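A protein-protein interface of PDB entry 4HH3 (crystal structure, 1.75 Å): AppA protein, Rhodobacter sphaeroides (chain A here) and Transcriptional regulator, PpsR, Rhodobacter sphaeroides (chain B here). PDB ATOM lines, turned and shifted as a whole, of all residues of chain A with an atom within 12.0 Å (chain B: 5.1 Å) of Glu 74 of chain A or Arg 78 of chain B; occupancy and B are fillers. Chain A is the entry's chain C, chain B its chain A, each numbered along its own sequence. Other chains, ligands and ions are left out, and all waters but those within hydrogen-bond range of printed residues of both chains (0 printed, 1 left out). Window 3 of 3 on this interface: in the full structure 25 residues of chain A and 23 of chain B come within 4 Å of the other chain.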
ATOM      1  N   SER A  29     -26.195 -14.130 -25.584  1.00  0.00           N
ATOM      2  CA  SER A  29     -25.831 -15.435 -26.128  1.00  0.00           C
ATOM      3  C   SER A  29     -26.720 -15.818 -27.302  1.00  0.00           C
ATOM      4  O   SER A  29     -26.243 -16.379 -28.296  1.00  0.00           O
ATOM      5  CB  SER A  29     -25.917 -16.520 -25.043  1.00  0.00           C
ATOM      6  OG  SER A  29     -24.978 -16.220 -24.032  1.00  0.00           O
ATOM      7  N   SER A  33     -25.552 -16.195 -31.262  1.00  0.00           N
ATOM      8  CA  SER A  33     -25.680 -17.543 -31.815  1.00  0.00           C
ATOM      9  C   SER A  33     -26.529 -17.614 -33.070  1.00  0.00           C
ATOM     10  O   SER A  33     -26.636 -18.675 -33.690  1.00  0.00           O
ATOM     11  CB  SER A  33     -26.313 -18.481 -30.785  1.00  0.00           C
ATOM     12  OG  SER A  33     -25.513 -18.599 -29.635  1.00  0.00           O
ATOM     13  N   CYS A  64     -21.028 -15.540 -21.639  1.00  0.00           N
ATOM     14  CA  CYS A  64     -21.535 -15.916 -22.959  1.00  0.00           C
ATOM     15  C   CYS A  64     -20.667 -16.969 -23.614  1.00  0.00           C
ATOM     16  O   CYS A  64     -21.187 -17.895 -24.244  1.00  0.00           O
ATOM     17  CB  CYS A  64     -21.638 -14.709 -23.862  1.00  0.00           C
ATOM     18  SG  CYS A  64     -22.939 -13.596 -23.295  1.00  0.00           S
ATOM     19  N   ALA A  65     -19.351 -16.846 -23.448  1.00  0.00           N
ATOM     20  CA  ALA A  65     -18.433 -17.818 -24.063  1.00  0.00           C
ATOM     21  C   ALA A  65     -18.649 -19.218 -23.507  1.00  0.00           C
ATOM     22  O   ALA A  65     -18.558 -20.210 -24.240  1.00  0.00           O
ATOM     23  CB  ALA A  65     -16.994 -17.401 -23.867  1.00  0.00           C
ATOM     24  N   GLU A  66     -18.944 -19.323 -22.214  1.00  0.00           N
ATOM     25  CA  GLU A  66     -19.273 -20.636 -21.655  1.00  0.00           C
ATOM     26  C   GLU A  66     -20.507 -21.240 -22.330  1.00  0.00           C
ATOM     27  O   GLU A  66     -20.553 -22.447 -22.598  1.00  0.00           O
ATOM     28  CB  GLU A  66     -19.466 -20.561 -20.132  1.00  0.00           C
ATOM     29  CG  GLU A  66     -18.169 -20.265 -19.387  1.00  0.00           C
ATOM     30  CD  GLU A  66     -18.348 -20.113 -17.882  1.00  0.00           C
ATOM     31  OE1 GLU A  66     -17.316 -20.016 -17.182  1.00  0.00           O
ATOM     32  OE2 GLU A  66     -19.510 -20.085 -17.408  1.00  0.00           O
ATOM     33  N   ARG A  67     -21.498 -20.401 -22.608  1.00  0.00           N
ATOM     34  CA  ARG A  67     -22.719 -20.854 -23.254  1.00  0.00           C
ATOM     35  C   ARG A  67     -22.474 -21.248 -24.708  1.00  0.00           C
ATOM     36  O   ARG A  67     -23.033 -22.236 -25.192  1.00  0.00           O
ATOM     37  CB  ARG A  67     -23.800 -19.783 -23.164  1.00  0.00           C
ATOM     38  CG  ARG A  67     -24.285 -19.561 -21.736  1.00  0.00           C
ATOM     39  CD  ARG A  67     -25.229 -18.390 -21.668  1.00  0.00           C
ATOM     40  NE  ARG A  67     -26.525 -18.690 -22.258  1.00  0.00           N
ATOM     41  CZ  ARG A  67     -27.577 -19.089 -21.552  1.00  0.00           C
ATOM     42  NH1 ARG A  67     -27.469 -19.247 -20.238  1.00  0.00           N
ATOM     43  NH2 ARG A  67     -28.731 -19.330 -22.151  1.00  0.00           N
ATOM     44  N   LEU A  68     -21.636 -20.478 -25.396  1.00  0.00           N
ATOM     45  CA  LEU A  68     -21.319 -20.782 -26.792  1.00  0.00           C
ATOM     46  C   LEU A  68     -20.521 -22.077 -26.883  1.00  0.00           C
ATOM     47  O   LEU A  68     -20.737 -22.895 -27.787  1.00  0.00           O
ATOM     48  CB  LEU A  68     -20.533 -19.637 -27.431  1.00  0.00           C
ATOM     49  CG  LEU A  68     -21.287 -18.320 -27.644  1.00  0.00           C
ATOM     50  CD1 LEU A  68     -20.332 -17.277 -28.210  1.00  0.00           C
ATOM     51  CD2 LEU A  68     -22.450 -18.522 -28.579  1.00  0.00           C
ATOM     52  N   THR A  69     -19.594 -22.253 -25.947  1.00  0.00           N
ATOM     53  CA  THR A  69     -18.791 -23.481 -25.877  1.00  0.00           C
ATOM     54  C   THR A  69     -19.675 -24.707 -25.705  1.00  0.00           C
ATOM     55  O   THR A  69     -19.483 -25.733 -26.377  1.00  0.00           O
ATOM     56  CB  THR A  69     -17.760 -23.388 -24.736  1.00  0.00           C
ATOM     57  OG1 THR A  69     -16.826 -22.341 -25.045  1.00  0.00           O
ATOM     58  CG2 THR A  69     -17.010 -24.705 -24.547  1.00  0.00           C
ATOM     59  N   ARG A  70     -20.657 -24.598 -24.819  1.00  0.00           N
ATOM     60  CA  ARG A  70     -21.611 -25.695 -24.616  1.00  0.00           C
ATOM     61  C   ARG A  70     -22.479 -25.948 -25.858  1.00  0.00           C
ATOM     62  O   ARG A  70     -22.729 -27.107 -26.228  1.00  0.00           O
ATOM     63  CB  ARG A  70     -22.474 -25.402 -23.386  1.00  0.00           C
ATOM     64  CG  ARG A  70     -23.597 -26.375 -23.110  1.00  0.00           C
ATOM     65  CD  ARG A  70     -24.240 -26.040 -21.756  1.00  0.00           C
ATOM     66  NE  ARG A  70     -23.239 -25.592 -20.785  1.00  0.00           N
ATOM     67  CZ  ARG A  70     -23.196 -24.379 -20.230  1.00  0.00           C
ATOM     68  NH1 ARG A  70     -24.113 -23.465 -20.525  1.00  0.00           N
ATOM     69  NH2 ARG A  70     -22.233 -24.081 -19.366  1.00  0.00           N
ATOM     70  N   ALA A  71     -22.924 -24.876 -26.511  1.00  0.00           N
ATOM     71  CA  ALA A  71     -23.760 -25.022 -27.699  1.00  0.00           C
ATOM     72  C   ALA A  71     -22.997 -25.727 -28.806  1.00  0.00           C
ATOM     73  O   ALA A  71     -23.557 -26.549 -29.535  1.00  0.00           O
ATOM     74  CB  ALA A  71     -24.274 -23.671 -28.180  1.00  0.00           C
ATOM     75  N   LEU A  72     -21.711 -25.421 -28.913  1.00  0.00           N
ATOM     76  CA  LEU A  72     -20.883 -26.030 -29.945  1.00  0.00           C
ATOM     77  C   LEU A  72     -20.711 -27.504 -29.618  1.00  0.00           C
ATOM     78  O   LEU A  72     -20.733 -28.359 -30.505  1.00  0.00           O
ATOM     79  CB  LEU A  72     -19.523 -25.344 -30.000  1.00  0.00           C
ATOM     80  CG  LEU A  72     -18.468 -25.850 -30.986  1.00  0.00           C
ATOM     81  CD1 LEU A  72     -19.000 -25.860 -32.417  1.00  0.00           C
ATOM     82  CD2 LEU A  72     -17.212 -24.985 -30.868  1.00  0.00           C
ATOM     83  N   ALA A  73     -20.545 -27.797 -28.330  1.00  0.00           N
ATOM     84  CA  ALA A  73     -20.393 -29.184 -27.876  1.00  0.00           C
ATOM     85  C   ALA A  73     -21.621 -30.049 -28.178  1.00  0.00           C
ATOM     86  O   ALA A  73     -21.506 -31.261 -28.419  1.00  0.00           O
ATOM     87  CB  ALA A  73     -20.057 -29.206 -26.375  1.00  0.00           C
ATOM     88  N   GLU A  74     -22.798 -29.433 -28.179  1.00  0.00           N
ATOM     89  CA  GLU A  74     -24.037 -30.158 -28.445  1.00  0.00           C
ATOM     90  C   GLU A  74     -24.463 -30.032 -29.912  1.00  0.00           C
ATOM     91  O   GLU A  74     -25.550 -30.469 -30.297  1.00  0.00           O
ATOM     92  CB  GLU A  74     -25.132 -29.647 -27.507  1.00  0.00           C
ATOM     93  CG  GLU A  74     -24.734 -29.767 -26.037  1.00  0.00           C
ATOM     94  CD  GLU A  74     -25.669 -29.040 -25.080  1.00  0.00           C
ATOM     95  OE1 GLU A  74     -25.481 -29.181 -23.850  1.00  0.00           O
ATOM     96  OE2 GLU A  74     -26.583 -28.329 -25.545  1.00  0.00           O
ATOM     97  N   ASP A  75     -23.581 -29.436 -30.713  1.00  0.00           N
ATOM     98  CA  ASP A  75     -23.821 -29.163 -32.136  1.00  0.00           C
ATOM     99  C   ASP A  75     -25.060 -28.318 -32.422  1.00  0.00           C
ATOM    100  O   ASP A  75     -25.672 -28.437 -33.484  1.00  0.00           O
ATOM    101  CB  ASP A  75     -23.810 -30.448 -32.965  1.00  0.00           C
ATOM    102  CG  ASP A  75     -22.421 -31.022 -33.099  1.00  0.00           C
ATOM    103  OD1 ASP A  75     -21.593 -30.421 -33.821  1.00  0.00           O
ATOM    104  OD2 ASP A  75     -22.151 -32.054 -32.462  1.00  0.00           O
ATOM    105  N   ARG A  76     -25.405 -27.437 -31.486  1.00  0.00           N
ATOM    106  CA  ARG A  76     -26.507 -26.516 -31.713  1.00  0.00           C
ATOM    107  C   ARG A  76     -26.027 -25.311 -32.534  1.00  0.00           C
ATOM    108  O   ARG A  76     -26.826 -24.633 -33.172  1.00  0.00           O
ATOM    109  CB  ARG A  76     -27.151 -26.105 -30.387  1.00  0.00           C
ATOM    110  CG  ARG A  76     -27.838 -27.287 -29.697  1.00  0.00           C
ATOM    111  CD  ARG A  76     -28.588 -26.882 -28.439  1.00  0.00           C
ATOM    112  NE  ARG A  76     -27.700 -26.731 -27.293  1.00  0.00           N
ATOM    113  CZ  ARG A  76     -27.290 -25.561 -26.814  1.00  0.00           C
ATOM    114  NH1 ARG A  76     -27.695 -24.430 -27.378  1.00  0.00           N
ATOM    115  NH2 ARG A  76     -26.485 -25.523 -25.758  1.00  0.00           N
ATOM    116  N   ILE A  77     -24.718 -25.067 -32.513  1.00  0.00           N
ATOM    117  CA  ILE A  77     -24.078 -24.091 -33.405  1.00  0.00           C
ATOM    118  C   ILE A  77     -22.774 -24.670 -33.943  1.00  0.00           C
ATOM    119  O   ILE A  77     -22.267 -25.669 -33.427  1.00  0.00           O
ATOM    120  CB  ILE A  77     -23.757 -22.736 -32.712  1.00  0.00           C
ATOM    121  CG1 ILE A  77     -22.718 -22.919 -31.601  1.00  0.00           C
ATOM    122  CG2 ILE A  77     -25.025 -22.056 -32.202  1.00  0.00           C
ATOM    123  CD1 ILE A  77     -22.432 -21.636 -30.802  1.00  0.00           C
ATOM    124  N   SER A  78     -22.245 -24.037 -34.985  1.00  0.00           N
ATOM    125  CA  SER A  78     -21.020 -24.473 -35.652  1.00  0.00           C
ATOM    126  C   SER A  78     -19.841 -23.567 -35.288  1.00  0.00           C
ATOM    127  O   SER A  78     -20.021 -22.473 -34.747  1.00  0.00           O
ATOM    128  CB  SER A  78     -21.226 -24.440 -37.173  1.00  0.00           C
ATOM    129  OG  SER A  78     -21.418 -23.095 -37.617  1.00  0.00           O
ATOM    130  N   ARG A  79     -18.627 -24.009 -35.590  1.00  0.00           N
ATOM    131  CA  ARG A  79     -17.455 -23.173 -35.349  1.00  0.00           C
ATOM    132  C   ARG A  79     -17.518 -21.922 -36.222  1.00  0.00           C
ATOM    133  O   ARG A  79     -17.107 -20.836 -35.792  1.00  0.00           O
ATOM    134  CB  ARG A  79     -16.153 -23.941 -35.614  1.00  0.00           C
ATOM    135  CG  ARG A  79     -14.881 -23.081 -35.593  1.00  0.00           C
ATOM    136  CD  ARG A  79     -14.730 -22.249 -34.314  1.00  0.00           C
ATOM    137  NE  ARG A  79     -14.458 -23.065 -33.132  1.00  0.00           N
ATOM    138  CZ  ARG A  79     -14.103 -22.570 -31.951  1.00  0.00           C
ATOM    139  NH1 ARG A  79     -13.869 -23.391 -30.939  1.00  0.00           N
ATOM    140  NH2 ARG A  79     -13.974 -21.255 -31.786  1.00  0.00           N
ATOM    141  N   GLN A  81     -20.201 -20.303 -36.892  1.00  0.00           N
ATOM    142  CA  GLN A  81     -21.073 -19.403 -36.139  1.00  0.00           C
ATOM    143  C   GLN A  81     -20.366 -18.743 -34.963  1.00  0.00           C
ATOM    144  O   GLN A  81     -20.592 -17.566 -34.686  1.00  0.00           O
ATOM    145  CB  GLN A  81     -22.333 -20.140 -35.668  1.00  0.00           C
ATOM    146  CG  GLN A  81     -23.319 -20.409 -36.805  1.00  0.00           C
ATOM    147  CD  GLN A  81     -24.493 -21.254 -36.362  1.00  0.00           C
ATOM    148  OE1 GLN A  81     -24.369 -22.464 -36.196  1.00  0.00           O
ATOM    149  NE2 GLN A  81     -25.642 -20.617 -36.163  1.00  0.00           N
ATOM    150  N   VAL A  82     -19.507 -19.492 -34.273  1.00  0.00           N
ATOM    151  CA  VAL A  82     -18.738 -18.916 -33.166  1.00  0.00           C
ATOM    152  C   VAL A  82     -17.787 -17.837 -33.690  1.00  0.00           C
ATOM    153  O   VAL A  82     -17.591 -16.794 -33.070  1.00  0.00           O
ATOM    154  CB  VAL A  82     -17.958 -20.010 -32.412  1.00  0.00           C
ATOM    155  CG1 VAL A  82     -17.046 -19.406 -31.353  1.00  0.00           C
ATOM    156  CG2 VAL A  82     -18.934 -20.991 -31.781  1.00  0.00           C
ATOM    157  N   LEU A 167     -12.683 -19.313 -26.225  1.00  0.00           N
ATOM    158  CA  LEU A 167     -13.480 -20.060 -27.200  1.00  0.00           C
ATOM    159  C   LEU A 167     -12.638 -21.059 -27.980  1.00  0.00           C
ATOM    160  O   LEU A 167     -13.052 -21.537 -29.036  1.00  0.00           O
ATOM    161  CB  LEU A 167     -14.195 -19.095 -28.159  1.00  0.00           C
ATOM    162  CG  LEU A 167     -15.348 -18.329 -27.498  1.00  0.00           C
ATOM    163  CD1 LEU A 167     -15.816 -17.161 -28.356  1.00  0.00           C
ATOM    164  CD2 LEU A 167     -16.502 -19.310 -27.227  1.00  0.00           C
ATOM    165  N   LYS B  74     -16.909 -35.115 -28.317  1.00  0.00           N
ATOM    166  CA  LYS B  74     -18.122 -35.029 -29.103  1.00  0.00           C
ATOM    167  C   LYS B  74     -18.405 -36.373 -29.796  1.00  0.00           C
ATOM    168  O   LYS B  74     -19.550 -36.817 -29.874  1.00  0.00           O
ATOM    169  CB  LYS B  74     -18.007 -33.902 -30.131  1.00  0.00           C
ATOM    170  CG  LYS B  74     -19.272 -33.664 -30.916  1.00  0.00           C
ATOM    171  CD  LYS B  74     -19.100 -32.493 -31.870  1.00  0.00           C
ATOM    172  CE  LYS B  74     -19.177 -31.164 -31.155  1.00  0.00           C
ATOM    173  NZ  LYS B  74     -19.235 -30.060 -32.168  1.00  0.00           N
ATOM    174  N   PHE B  75     -17.359 -37.011 -30.298  1.00  0.00           N
ATOM    175  CA  PHE B  75     -17.544 -38.327 -30.920  1.00  0.00           C
ATOM    176  C   PHE B  75     -18.071 -39.340 -29.902  1.00  0.00           C
ATOM    177  O   PHE B  75     -18.983 -40.118 -30.201  1.00  0.00           O
ATOM    178  CB  PHE B  75     -16.256 -38.841 -31.556  1.00  0.00           C
ATOM    179  CG  PHE B  75     -16.394 -40.226 -32.150  1.00  0.00           C
ATOM    180  CD1 PHE B  75     -16.953 -40.397 -33.403  1.00  0.00           C
ATOM    181  CD2 PHE B  75     -15.989 -41.346 -31.440  1.00  0.00           C
ATOM    182  CE1 PHE B  75     -17.096 -41.653 -33.949  1.00  0.00           C
ATOM    183  CE2 PHE B  75     -16.131 -42.606 -31.979  1.00  0.00           C
ATOM    184  CZ  PHE B  75     -16.687 -42.759 -33.234  1.00  0.00           C
ATOM    185  N   ARG B  76     -17.497 -39.331 -28.703  1.00  0.00           N
ATOM    186  CA  ARG B  76     -17.930 -40.250 -27.653  1.00  0.00           C
ATOM    187  C   ARG B  76     -19.375 -39.959 -27.253  1.00  0.00           C
ATOM    188  O   ARG B  76     -20.168 -40.876 -27.061  1.00  0.00           O
ATOM    189  CB  ARG B  76     -17.009 -40.166 -26.432  1.00  0.00           C
ATOM    190  CG  ARG B  76     -15.558 -40.527 -26.706  1.00  0.00           C
ATOM    191  CD  ARG B  76     -14.730 -40.472 -25.427  1.00  0.00           C
ATOM    192  NE  ARG B  76     -13.327 -40.802 -25.659  1.00  0.00           N
ATOM    193  CZ  ARG B  76     -12.399 -40.828 -24.708  1.00  0.00           C
ATOM    194  NH1 ARG B  76     -12.725 -40.548 -23.454  1.00  0.00           N
ATOM    195  NH2 ARG B  76     -11.146 -41.138 -25.010  1.00  0.00           N
ATOM    196  N   LEU B  77     -19.712 -38.676 -27.144  1.00  0.00           N
ATOM    197  CA  LEU B  77     -21.057 -38.250 -26.770  1.00  0.00           C
ATOM    198  C   LEU B  77     -22.138 -38.803 -27.703  1.00  0.00           C
ATOM    199  O   LEU B  77     -23.167 -39.307 -27.250  1.00  0.00           O
ATOM    200  CB  LEU B  77     -21.134 -36.715 -26.739  1.00  0.00           C
ATOM    201  CG  LEU B  77     -22.469 -36.065 -26.368  1.00  0.00           C
ATOM    202  CD1 LEU B  77     -22.797 -36.283 -24.897  1.00  0.00           C
ATOM    203  CD2 LEU B  77     -22.465 -34.568 -26.706  1.00  0.00           C
ATOM    204  N   ARG B  78     -21.900 -38.714 -29.007  1.00  0.00           N
ATOM    205  CA  ARG B  78     -22.922 -39.086 -29.976  1.00  0.00           C
ATOM    206  C   ARG B  78     -22.827 -40.542 -30.421  1.00  0.00           C
ATOM    207  O   ARG B  78     -23.694 -41.022 -31.148  1.00  0.00           O
ATOM    208  CB  ARG B  78     -22.866 -38.162 -31.188  1.00  0.00           C
ATOM    209  CG  ARG B  78     -23.066 -36.708 -30.826  1.00  0.00           C
ATOM    210  CD  ARG B  78     -24.407 -36.487 -30.157  1.00  0.00           C
ATOM    211  NE  ARG B  78     -24.726 -35.064 -30.045  1.00  0.00           N
ATOM    212  CZ  ARG B  78     -25.729 -34.578 -29.323  1.00  0.00           C
ATOM    213  NH1 ARG B  78     -26.512 -35.396 -28.633  1.00  0.00           N
ATOM    214  NH2 ARG B  78     -25.944 -33.269 -29.281  1.00  0.00           N
ATOM    215  N   SER B  79     -21.781 -41.237 -29.989  1.00  0.00           N
ATOM    216  CA  SER B  79     -21.604 -42.625 -30.405  1.00  0.00           C
ATOM    217  C   SER B  79     -21.857 -43.624 -29.285  1.00  0.00           C
ATOM    218  O   SER B  79     -22.313 -44.737 -29.537  1.00  0.00           O
ATOM    219  CB  SER B  79     -20.216 -42.847 -31.012  1.00  0.00           C
ATOM    220  OG  SER B  79     -19.208 -42.770 -30.023  1.00  0.00           O
ATOM    221  N   GLU B  80     -21.570 -43.235 -28.047  1.00  0.00           N
ATOM    222  CA  GLU B  80     -21.667 -44.187 -26.938  1.00  0.00           C
ATOM    223  C   GLU B  80     -23.070 -44.769 -26.707  1.00  0.00           C
ATOM    224  O   GLU B  80     -23.204 -45.934 -26.329  1.00  0.00           O
ATOM    225  CB  GLU B  80     -21.067 -43.608 -25.653  1.00  0.00           C
ATOM    226  CG  GLU B  80     -19.543 -43.691 -25.626  1.00  0.00           C
ATOM    227  CD  GLU B  80     -18.923 -42.983 -24.434  1.00  0.00           C
ATOM    228  OE1 GLU B  80     -19.672 -42.407 -23.615  1.00  0.00           O
ATOM    229  OE2 GLU B  80     -17.680 -43.001 -24.320  1.00  0.00           O
ATOM    230  N   GLY B  81     -24.109 -43.976 -26.939  1.00  0.00           N
ATOM    231  CA  GLY B  81     -25.466 -44.489 -26.850  1.00  0.00           C
ATOM    232  C   GLY B  81     -26.104 -44.790 -28.199  1.00  0.00           C
ATOM    233  O   GLY B  81     -27.297 -45.078 -28.277  1.00  0.00           O
ATOM    234  N   LEU B  82     -25.309 -44.730 -29.264  1.00  0.00           N
ATOM    235  CA  LEU B  82     -25.836 -44.865 -30.619  1.00  0.00           C
ATOM    236  C   LEU B  82     -26.146 -46.312 -31.006  1.00  0.00           C
ATOM    237  O   LEU B  82     -25.252 -47.154 -31.073  1.00  0.00           O
ATOM    238  CB  LEU B  82     -24.860 -44.256 -31.630  1.00  0.00           C
ATOM    239  CG  LEU B  82     -25.296 -44.264 -33.095  1.00  0.00           C
ATOM    240  CD1 LEU B  82     -26.495 -43.341 -33.304  1.00  0.00           C
ATOM    241  CD2 LEU B  82     -24.135 -43.877 -34.022  1.00  0.00           C
ATOM    242  N   SER B  88     -27.004 -40.484 -36.273  1.00  0.00           N
ATOM    243  CA  SER B  88     -26.860 -39.513 -35.197  1.00  0.00           C
ATOM    244  C   SER B  88     -27.272 -38.151 -35.716  1.00  0.00           C
ATOM    245  O   SER B  88     -27.463 -37.966 -36.917  1.00  0.00           O
ATOM    246  CB  SER B  88     -25.401 -39.436 -34.747  1.00  0.00           C
ATOM    247  OG  SER B  88     -24.612 -38.766 -35.728  1.00  0.00           O
ATOM    248  N   VAL B  89     -27.397 -37.183 -34.815  1.00  0.00           N
ATOM    249  CA  VAL B  89     -27.509 -35.800 -35.250  1.00  0.00           C
ATOM    250  C   VAL B  89     -26.175 -35.463 -35.896  1.00  0.00           C
ATOM    251  O   VAL B  89     -25.164 -36.106 -35.604  1.00  0.00           O
ATOM    252  CB  VAL B  89     -27.772 -34.843 -34.074  1.00  0.00           C
ATOM    253  CG1 VAL B  89     -29.059 -35.225 -33.358  1.00  0.00           C
ATOM    254  CG2 VAL B  89     -26.598 -34.852 -33.107  1.00  0.00           C
ATOM    255  N   VAL B  91     -22.650 -34.117 -36.621  1.00  0.00           N
ATOM    256  CA  VAL B  91     -21.575 -33.717 -35.724  1.00  0.00           C
ATOM    257  C   VAL B  91     -20.409 -33.113 -36.469  1.00  0.00           C
ATOM    258  O   VAL B  91     -19.897 -33.649 -37.445  1.00  0.00           O
ATOM    259  CB  VAL B  91     -21.088 -34.845 -34.784  1.00  0.00           C
ATOM    260  CG1 VAL B  91     -22.195 -35.233 -33.838  1.00  0.00           C
ATOM    261  CG2 VAL B  91     -20.591 -36.047 -35.580  1.00  0.00           C
ATOM    262  N   LEU B 109     -23.256 -40.146 -38.006  1.00  0.00           N
ATOM    263  CA  LEU B 109     -22.767 -41.458 -37.546  1.00  0.00           C
ATOM    264  C   LEU B 109     -23.864 -42.497 -37.631  1.00  0.00           C
ATOM    265  O   LEU B 109     -25.010 -42.220 -37.284  1.00  0.00           O
ATOM    266  CB  LEU B 109     -22.270 -41.390 -36.094  1.00  0.00           C
ATOM    267  CG  LEU B 109     -21.436 -40.162 -35.728  1.00  0.00           C
ATOM    268  CD1 LEU B 109     -21.129 -40.154 -34.235  1.00  0.00           C
ATOM    269  CD2 LEU B 109     -20.154 -40.108 -36.546  1.00  0.00           C
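Of the printed residues of chain B, Glu 74 of chain A touches Arg 78. Arg 78 of chain B touches just one residue of chain A: Glu 74. Of the printed residues of chain A, Lys 74 of chain B touches Leu 72, Ala 73 and Asp 75. Phe 75 of chain B touches none of the printed residues of chain A. Of chain A, only Ala 73 (3.8 Å) comes within 4 Å of Leu 77 of chain B. No residue of chain A comes within 4 Å of Ser 79 of chain B. No residue of chain A comes within 4 Å of Glu 80 of chain B. No residue of chain A comes within 4 Å of Leu 82 of chain B. No residue of chain A comes within 4 Å of Ser 88 of chain B. No residue of chain A comes within 4 Å of Val 89 of chain B. No residue of chain A comes within 4 Å of Leu 109 of chain B. Of the printed residues of chain B, Ala 73 of chain A touches Lys 74 (3.6 Å) and Leu 77 (3.8 Å). Printed residues of chain B within 4 Å of Leu 72 of chain A: Lys 74. Of the printed residues of chain A, Val 91 of chain B touches Asp 75. Printed residues of chain B within 4 Å of Asp 75 of chain A: Lys 74 and Val 91. Leu 68 of chain A touches none of the printed residues of chain B. The nearest printed residue of chain B that does not touch Glu 74 of chain A is Leu 77 of chain B (5.0 Å). The nearest residue of chain A that does not touch Arg 78 of chain B is Asp 75 of chain A (4.6 Å). The nearest printed residue of chain B that does not touch Asp 75 of chain A is Arg 78 of chain B (4.6 Å).
NH2 of Arg 78 of chain B is in hydrogen-bond range of O of Glu 74 of chain A (3.0 Å). NZ of Lys 74 of chain B lies within salt-bridge range of OD1 of Asp 75 of chain A (2.9 Å). NZ of Lys 74 of chain B lies within hydrogen-bond range of O of Leu 72 of chain A, at 2.8 Å.
Of the 21 printed residues of chain A, 4 touch a printed residue of chain B. Of the 13 printed residues of chain B, 4 touch a printed residue of chain A. Printed residues of chain B that touch a printed residue of chain A: Lys 74, Leu 77, Arg 78 and Val 91. Hydrophobic or aromatic side chains of chain B that line the printed part of chain A: Leu 77 and Val 91. Among the printed residues, 6 pairs touch across the chains. Among the printed residues, Asp or Glu carboxylates within 4 Å of a Lys or Arg side-chain nitrogen of the other chain: Asp 75 of chain A with Lys 74 of chain B (2.9 Å).
Among the printed residues, pairs that only touch across the chains: Asp 75 of chain A with Val 91 of chain B, Ala 73 of chain A with Lys 74 of chain B and Ala 73 of chain A with Leu 77 of chain B.
OE2 of Glu 74 of chain A lies within salt-bridge range of NE of Arg 76 of chain A (2.6 Å).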
